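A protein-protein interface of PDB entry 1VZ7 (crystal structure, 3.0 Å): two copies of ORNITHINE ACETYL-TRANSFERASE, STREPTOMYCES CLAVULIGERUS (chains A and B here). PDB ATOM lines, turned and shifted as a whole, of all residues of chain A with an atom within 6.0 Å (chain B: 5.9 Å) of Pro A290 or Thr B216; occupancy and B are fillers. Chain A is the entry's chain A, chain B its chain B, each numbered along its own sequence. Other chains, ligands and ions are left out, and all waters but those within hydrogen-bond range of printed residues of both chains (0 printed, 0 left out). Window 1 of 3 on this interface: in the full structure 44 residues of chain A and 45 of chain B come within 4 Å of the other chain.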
ATOM      1  N   VAL A 286      -5.626   4.242 -12.919  1.00  0.00           N
ATOM      2  CA  VAL A 286      -5.734   4.655 -14.320  1.00  0.00           C
ATOM      3  C   VAL A 286      -6.212   3.504 -15.197  1.00  0.00           C
ATOM      4  O   VAL A 286      -7.185   3.636 -15.934  1.00  0.00           O
ATOM      5  CB  VAL A 286      -4.361   5.169 -14.867  1.00  0.00           C
ATOM      6  CG1 VAL A 286      -4.408   5.339 -16.367  1.00  0.00           C
ATOM      7  CG2 VAL A 286      -4.025   6.494 -14.244  1.00  0.00           C
ATOM      8  N   ASN A 288      -7.636   0.783 -14.301  1.00  0.00           N
ATOM      9  CA  ASN A 288      -8.915   0.204 -13.909  1.00  0.00           C
ATOM     10  C   ASN A 288     -10.082   1.178 -14.068  1.00  0.00           C
ATOM     11  O   ASN A 288     -11.239   0.797 -13.913  1.00  0.00           O
ATOM     12  CB  ASN A 288      -8.878  -0.293 -12.469  1.00  0.00           C
ATOM     13  CG  ASN A 288      -7.966  -1.472 -12.288  1.00  0.00           C
ATOM     14  OD1 ASN A 288      -7.902  -2.352 -13.141  1.00  0.00           O
ATOM     15  ND2 ASN A 288      -7.260  -1.507 -11.164  1.00  0.00           N
ATOM     16  N   SER A 289      -9.788   2.433 -14.376  1.00  0.00           N
ATOM     17  CA  SER A 289     -10.855   3.410 -14.548  1.00  0.00           C
ATOM     18  C   SER A 289     -11.724   3.065 -15.741  1.00  0.00           C
ATOM     19  O   SER A 289     -11.270   3.130 -16.872  1.00  0.00           O
ATOM     20  CB  SER A 289     -10.280   4.810 -14.747  1.00  0.00           C
ATOM     21  OG  SER A 289     -11.294   5.709 -15.153  1.00  0.00           O
ATOM     22  N   PRO A 290     -12.990   2.701 -15.508  1.00  0.00           N
ATOM     23  CA  PRO A 290     -13.859   2.364 -16.639  1.00  0.00           C
ATOM     24  C   PRO A 290     -13.824   3.461 -17.698  1.00  0.00           C
ATOM     25  O   PRO A 290     -13.739   3.176 -18.894  1.00  0.00           O
ATOM     26  CB  PRO A 290     -15.233   2.229 -15.995  1.00  0.00           C
ATOM     27  CG  PRO A 290     -14.905   1.790 -14.622  1.00  0.00           C
ATOM     28  CD  PRO A 290     -13.740   2.652 -14.245  1.00  0.00           C
ATOM     29  N   LEU A 291     -13.886   4.715 -17.253  1.00  0.00           N
ATOM     30  CA  LEU A 291     -13.861   5.836 -18.180  1.00  0.00           C
ATOM     31  C   LEU A 291     -12.569   5.844 -18.987  1.00  0.00           C
ATOM     32  O   LEU A 291     -12.598   6.086 -20.196  1.00  0.00           O
ATOM     33  CB  LEU A 291     -14.056   7.161 -17.439  1.00  0.00           C
ATOM     34  CG  LEU A 291     -15.507   7.602 -17.186  1.00  0.00           C
ATOM     35  CD1 LEU A 291     -15.555   8.844 -16.305  1.00  0.00           C
ATOM     36  CD2 LEU A 291     -16.176   7.878 -18.519  1.00  0.00           C
ATOM     37  N   VAL A 292     -11.434   5.573 -18.341  1.00  0.00           N
ATOM     38  CA  VAL A 292     -10.181   5.524 -19.078  1.00  0.00           C
ATOM     39  C   VAL A 292     -10.295   4.312 -19.979  1.00  0.00           C
ATOM     40  O   VAL A 292     -10.207   4.427 -21.193  1.00  0.00           O
ATOM     41  CB  VAL A 292      -8.971   5.348 -18.164  1.00  0.00           C
ATOM     42  CG1 VAL A 292      -7.720   5.174 -18.999  1.00  0.00           C
ATOM     43  CG2 VAL A 292      -8.804   6.562 -17.303  1.00  0.00           C
ATOM     44  N   LYS A 293     -10.528   3.155 -19.363  1.00  0.00           N
ATOM     45  CA  LYS A 293     -10.673   1.883 -20.070  1.00  0.00           C
ATOM     46  C   LYS A 293     -11.602   1.943 -21.278  1.00  0.00           C
ATOM     47  O   LYS A 293     -11.441   1.166 -22.223  1.00  0.00           O
ATOM     48  CB  LYS A 293     -11.186   0.809 -19.124  1.00  0.00           C
ATOM     49  CG  LYS A 293     -10.220   0.410 -18.022  1.00  0.00           C
ATOM     50  CD  LYS A 293     -10.910  -0.554 -17.049  1.00  0.00           C
ATOM     51  CE  LYS A 293     -11.399  -1.818 -17.743  1.00  0.00           C
ATOM     52  NZ  LYS A 293     -10.323  -2.835 -17.767  1.00  0.00           N
ATOM     53  N   THR A 294     -12.568   2.862 -21.257  1.00  0.00           N
ATOM     54  CA  THR A 294     -13.502   2.989 -22.369  1.00  0.00           C
ATOM     55  C   THR A 294     -13.027   3.895 -23.498  1.00  0.00           C
ATOM     56  O   THR A 294     -13.387   3.679 -24.644  1.00  0.00           O
ATOM     57  CB  THR A 294     -14.897   3.467 -21.891  1.00  0.00           C
ATOM     58  OG1 THR A 294     -14.756   4.561 -20.976  1.00  0.00           O
ATOM     59  CG2 THR A 294     -15.647   2.327 -21.234  1.00  0.00           C
ATOM     60  N   ALA A 295     -12.229   4.910 -23.182  1.00  0.00           N
ATOM     61  CA  ALA A 295     -11.708   5.815 -24.215  1.00  0.00           C
ATOM     62  C   ALA A 295     -10.608   5.096 -25.010  1.00  0.00           C
ATOM     63  O   ALA A 295     -10.437   5.316 -26.205  1.00  0.00           O
ATOM     64  CB  ALA A 295     -11.154   7.084 -23.576  1.00  0.00           C
ATOM     65  N   MET A 308      -8.318  12.814 -14.553  1.00  0.00           N
ATOM     66  CA  MET A 308      -9.355  12.605 -13.550  1.00  0.00           C
ATOM     67  C   MET A 308      -9.087  11.321 -12.760  1.00  0.00           C
ATOM     68  O   MET A 308      -9.210  11.293 -11.534  1.00  0.00           O
ATOM     69  CB  MET A 308     -10.718  12.586 -14.252  1.00  0.00           C
ATOM     70  CG  MET A 308     -11.853  11.958 -13.477  1.00  0.00           C
ATOM     71  SD  MET A 308     -11.905  10.152 -13.612  1.00  0.00           S
ATOM     72  CE  MET A 308     -12.156   9.772 -11.986  1.00  0.00           C
ATOM     73  N   LYS A 312      -7.891  10.781  -8.980  1.00  0.00           N
ATOM     74  CA  LYS A 312      -8.726   9.958  -8.130  1.00  0.00           C
ATOM     75  C   LYS A 312      -8.018   9.481  -6.849  1.00  0.00           C
ATOM     76  O   LYS A 312      -8.680   9.152  -5.865  1.00  0.00           O
ATOM     77  CB  LYS A 312      -9.229   8.751  -8.928  1.00  0.00           C
ATOM     78  CG  LYS A 312     -10.711   8.508  -8.801  1.00  0.00           C
ATOM     79  CD  LYS A 312     -11.091   7.083  -9.200  1.00  0.00           C
ATOM     80  CE  LYS A 312     -11.128   6.850 -10.704  1.00  0.00           C
ATOM     81  NZ  LYS A 312     -11.728   5.512 -10.992  1.00  0.00           N
ATOM     82  N   LEU A 380     -12.114  -1.671 -21.942  1.00  0.00           N
ATOM     83  CA  LEU A 380     -13.376  -2.330 -21.653  1.00  0.00           C
ATOM     84  C   LEU A 380     -14.280  -2.223 -22.874  1.00  0.00           C
ATOM     85  O   LEU A 380     -14.756  -1.144 -23.203  1.00  0.00           O
ATOM     86  CB  LEU A 380     -14.035  -1.653 -20.451  1.00  0.00           C
ATOM     87  CG  LEU A 380     -15.557  -1.730 -20.374  1.00  0.00           C
ATOM     88  CD1 LEU A 380     -15.987  -3.050 -19.775  1.00  0.00           C
ATOM     89  CD2 LEU A 380     -16.059  -0.581 -19.540  1.00  0.00           C
ATOM     90  N   LEU B 175     -19.114   9.268 -11.895  1.00  0.00           N
ATOM     91  CA  LEU B 175     -19.761   9.539 -10.636  1.00  0.00           C
ATOM     92  C   LEU B 175     -19.631   8.532  -9.506  1.00  0.00           C
ATOM     93  O   LEU B 175     -20.200   7.446  -9.542  1.00  0.00           O
ATOM     94  CB  LEU B 175     -21.240   9.829 -10.894  1.00  0.00           C
ATOM     95  CG  LEU B 175     -21.981  10.479  -9.732  1.00  0.00           C
ATOM     96  CD1 LEU B 175     -23.303  11.016 -10.231  1.00  0.00           C
ATOM     97  CD2 LEU B 175     -22.190   9.484  -8.600  1.00  0.00           C
ATOM     98  N   GLU B 176     -18.859   8.929  -8.504  1.00  0.00           N
ATOM     99  CA  GLU B 176     -18.663   8.176  -7.285  1.00  0.00           C
ATOM    100  C   GLU B 176     -18.095   9.212  -6.342  1.00  0.00           C
ATOM    101  O   GLU B 176     -16.892   9.279  -6.131  1.00  0.00           O
ATOM    102  CB  GLU B 176     -17.683   7.028  -7.435  1.00  0.00           C
ATOM    103  CG  GLU B 176     -17.441   6.367  -6.093  1.00  0.00           C
ATOM    104  CD  GLU B 176     -16.453   5.225  -6.147  1.00  0.00           C
ATOM    105  OE1 GLU B 176     -15.275   5.450  -6.537  1.00  0.00           O
ATOM    106  OE2 GLU B 176     -16.863   4.096  -5.788  1.00  0.00           O
ATOM    107  N   SER B 213     -22.499   4.971  -6.507  1.00  0.00           N
ATOM    108  CA  SER B 213     -21.399   4.811  -7.440  1.00  0.00           C
ATOM    109  C   SER B 213     -21.831   4.158  -8.744  1.00  0.00           C
ATOM    110  O   SER B 213     -22.326   3.037  -8.749  1.00  0.00           O
ATOM    111  CB  SER B 213     -20.296   3.979  -6.797  1.00  0.00           C
ATOM    112  OG  SER B 213     -19.281   3.670  -7.739  1.00  0.00           O
ATOM    113  N   ILE B 214     -21.614   4.875  -9.844  1.00  0.00           N
ATOM    114  CA  ILE B 214     -21.946   4.422 -11.188  1.00  0.00           C
ATOM    115  C   ILE B 214     -20.774   3.668 -11.835  1.00  0.00           C
ATOM    116  O   ILE B 214     -20.939   2.542 -12.325  1.00  0.00           O
ATOM    117  CB  ILE B 214     -22.274   5.616 -12.077  1.00  0.00           C
ATOM    118  CG1 ILE B 214     -23.461   6.389 -11.492  1.00  0.00           C
ATOM    119  CG2 ILE B 214     -22.518   5.149 -13.503  1.00  0.00           C
ATOM    120  CD1 ILE B 214     -24.813   5.670 -11.587  1.00  0.00           C
ATOM    121  N   ASP B 215     -19.596   4.296 -11.831  1.00  0.00           N
ATOM    122  CA  ASP B 215     -18.384   3.721 -12.422  1.00  0.00           C
ATOM    123  C   ASP B 215     -17.101   3.940 -11.619  1.00  0.00           C
ATOM    124  O   ASP B 215     -16.014   3.803 -12.157  1.00  0.00           O
ATOM    125  CB  ASP B 215     -18.168   4.288 -13.822  1.00  0.00           C
ATOM    126  CG  ASP B 215     -18.280   5.787 -13.857  1.00  0.00           C
ATOM    127  OD1 ASP B 215     -18.031   6.421 -12.808  1.00  0.00           O
ATOM    128  OD2 ASP B 215     -18.608   6.333 -14.930  1.00  0.00           O
ATOM    129  N   THR B 216     -17.229   4.280 -10.341  1.00  0.00           N
ATOM    130  CA  THR B 216     -16.082   4.517  -9.457  1.00  0.00           C
ATOM    131  C   THR B 216     -15.217   5.699  -9.875  1.00  0.00           C
ATOM    132  O   THR B 216     -14.159   5.910  -9.290  1.00  0.00           O
ATOM    133  CB  THR B 216     -15.106   3.300  -9.368  1.00  0.00           C
ATOM    134  OG1 THR B 216     -14.350   3.214 -10.580  1.00  0.00           O
ATOM    135  CG2 THR B 216     -15.837   2.007  -9.134  1.00  0.00           C
ATOM    136  N   ASP B 217     -15.646   6.468 -10.869  1.00  0.00           N
ATOM    137  CA  ASP B 217     -14.829   7.586 -11.315  1.00  0.00           C
ATOM    138  C   ASP B 217     -15.056   8.918 -10.627  1.00  0.00           C
ATOM    139  O   ASP B 217     -15.553   9.858 -11.240  1.00  0.00           O
ATOM    140  CB  ASP B 217     -14.956   7.784 -12.831  1.00  0.00           C
ATOM    141  CG  ASP B 217     -14.103   6.805 -13.621  1.00  0.00           C
ATOM    142  OD1 ASP B 217     -12.956   6.568 -13.203  1.00  0.00           O
ATOM    143  OD2 ASP B 217     -14.571   6.281 -14.658  1.00  0.00           O
ATOM    144  N   THR B 218     -14.660   9.011  -9.364  1.00  0.00           N
ATOM    145  CA  THR B 218     -14.806  10.254  -8.630  1.00  0.00           C
ATOM    146  C   THR B 218     -14.387  11.437  -9.476  1.00  0.00           C
ATOM    147  O   THR B 218     -13.222  11.565  -9.838  1.00  0.00           O
ATOM    148  CB  THR B 218     -13.941  10.285  -7.413  1.00  0.00           C
ATOM    149  OG1 THR B 218     -14.540   9.496  -6.394  1.00  0.00           O
ATOM    150  CG2 THR B 218     -13.788  11.717  -6.925  1.00  0.00           C
ATOM    151  N   ASN B 288     -19.445  -2.152  -7.255  1.00  0.00           N
ATOM    152  CA  ASN B 288     -18.535  -1.709  -8.314  1.00  0.00           C
ATOM    153  C   ASN B 288     -17.916  -2.880  -9.079  1.00  0.00           C
ATOM    154  O   ASN B 288     -17.267  -2.693 -10.108  1.00  0.00           O
ATOM    155  CB  ASN B 288     -17.428  -0.828  -7.755  1.00  0.00           C
ATOM    156  CG  ASN B 288     -17.944   0.495  -7.304  1.00  0.00           C
ATOM    157  OD1 ASN B 288     -18.725   1.131  -7.998  1.00  0.00           O
ATOM    158  ND2 ASN B 288     -17.512   0.929  -6.135  1.00  0.00           N
ATOM    159  N   TYR B 384     -23.053   1.944 -21.732  1.00  0.00           N
ATOM    160  CA  TYR B 384     -22.036   2.749 -21.059  1.00  0.00           C
ATOM    161  C   TYR B 384     -20.735   2.673 -21.844  1.00  0.00           C
ATOM    162  O   TYR B 384     -20.039   3.671 -22.019  1.00  0.00           O
ATOM    163  CB  TYR B 384     -21.804   2.257 -19.629  1.00  0.00           C
ATOM    164  CG  TYR B 384     -20.704   2.996 -18.895  1.00  0.00           C
ATOM    165  CD1 TYR B 384     -19.354   2.765 -19.189  1.00  0.00           C
ATOM    166  CD2 TYR B 384     -21.007   3.935 -17.919  1.00  0.00           C
ATOM    167  CE1 TYR B 384     -18.343   3.452 -18.524  1.00  0.00           C
ATOM    168  CE2 TYR B 384     -20.000   4.622 -17.256  1.00  0.00           C
ATOM    169  CZ  TYR B 384     -18.675   4.373 -17.563  1.00  0.00           C
ATOM    170  OH  TYR B 384     -17.685   5.038 -16.886  1.00  0.00           O
ATOM    171  N   ASN B 388     -19.264   6.070 -23.619  1.00  0.00           N
ATOM    172  CA  ASN B 388     -17.992   6.605 -23.149  1.00  0.00           C
ATOM    173  C   ASN B 388     -16.846   6.139 -24.011  1.00  0.00           C
ATOM    174  O   ASN B 388     -15.725   5.972 -23.546  1.00  0.00           O
ATOM    175  CB  ASN B 388     -17.729   6.209 -21.700  1.00  0.00           C
ATOM    176  CG  ASN B 388     -18.465   7.082 -20.718  1.00  0.00           C
ATOM    177  OD1 ASN B 388     -18.399   8.310 -20.790  1.00  0.00           O
ATOM    178  ND2 ASN B 388     -19.168   6.453 -19.783  1.00  0.00           N
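Of the 12 printed residues of chain A, 7 touch a printed residue of chain B. Of the 11 printed residues of chain B, 6 touch a printed residue of chain A. Hydrophobic or aromatic side chains of chain B within 4 Å of the printed part of chain A: Tyr B384.
SD of Met A308 lies close to OD1 of Asp B217, 3.8 Å away. The side-chain carboxylate (OD1) of Asp B217 is in salt-bridge range of the side-chain amino group (NZ) of Lys A312 (2.7 Å). OG of Ser A289 lies within hydrogen-bond range of OD1 of Asp B217 (2.7 Å). OG1 of Thr A294 lies within hydrogen-bond range of O of Asn B388 (3.1 Å). The side-chain amino group (NZ) of Lys A312 sits at hydrogen-bond distance from the backbone carbonyl oxygen (O) of Thr B216, at 3.0 Å. The side-chain carboxylate of Asp B217 sits close to the backbone NH of Leu A291 (3.1 Å).
The backbone NH (N) of Leu B175 is in hydrogen-bond range of the side-chain carboxylate (OD1) of Asp B215, at 3.2 Å. The side-chain carboxylate (OD2) of Asp B215 lies within hydrogen-bond range of the side-chain hydroxyl (OH) of Tyr B384, at 2.5 Å. The backbone NH (N) of Val A292 is in hydrogen-bond range of the side-chain hydroxyl (OG) of Ser A289 (3.2 Å). O of Pro A290 sits at hydrogen-bond distance from OG1 of Thr A294 (2.7 Å). The backbone carbonyl oxygen of Leu A291 lies within hydrogen-bond range of the side-chain hydroxyl of Thr A294 (2.8 Å). N of Leu A291 lies close to OG of Ser A289.
Among the printed residues, merely in contact across the chains: Met A308 with Thr B218, Leu A291 with Asn B388, Pro A290 with Asp B215, Leu A291 with Tyr B384, Ala A295 with Asn B388, Pro A290 with Asp B217, Pro A290 with Thr B216, Pro A290 with Tyr B384, Lys A312 with Thr B218 and Thr A294 with Tyr B384.
1 position is printed for both chains. Of the 16 pairs that touch across the chains among the printed residues, none has its exchanged pair printed and touching as well.
Of chain B, only Asp B215 (3.3 Å), Thr B216 (3.8 Å), Asp B217 (3.7 Å) and Tyr B384 (3.8 Å) come within 4 Å of Pro A290. Of the printed residues of chain B, Thr A294 touches Tyr B384 (3.98 Å) and Asn B388 (3.1 Å). Printed residues of chain B within 4 Å of Met A308: Asp B217 (3.3 Å) and Thr B218 (3.0 Å). Of the printed residues of chain B, Lys A312 touches Thr B216, Asp B217 and Thr B218. Of chain A, only Pro A290 (3.8 Å) and Lys A312 (3.0 Å) come within 4 Å of Thr B216. Printed residues of chain A within 4 Å of Asp B217: Ser A289, Pro A290, Leu A291, Met A308 and Lys A312. Of the printed residues of chain A, Thr B218 touches Met A308 and Lys A312. The nearest residue of chain B that does not touch Pro A290 is Asn B388 (5.7 Å). The nearest residue of chain A that does not touch Thr B216 is Met A308 (5.1 Å). The nearest printed residue of chain A that does not touch Asp B217 is Val A292 (4.9 Å).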
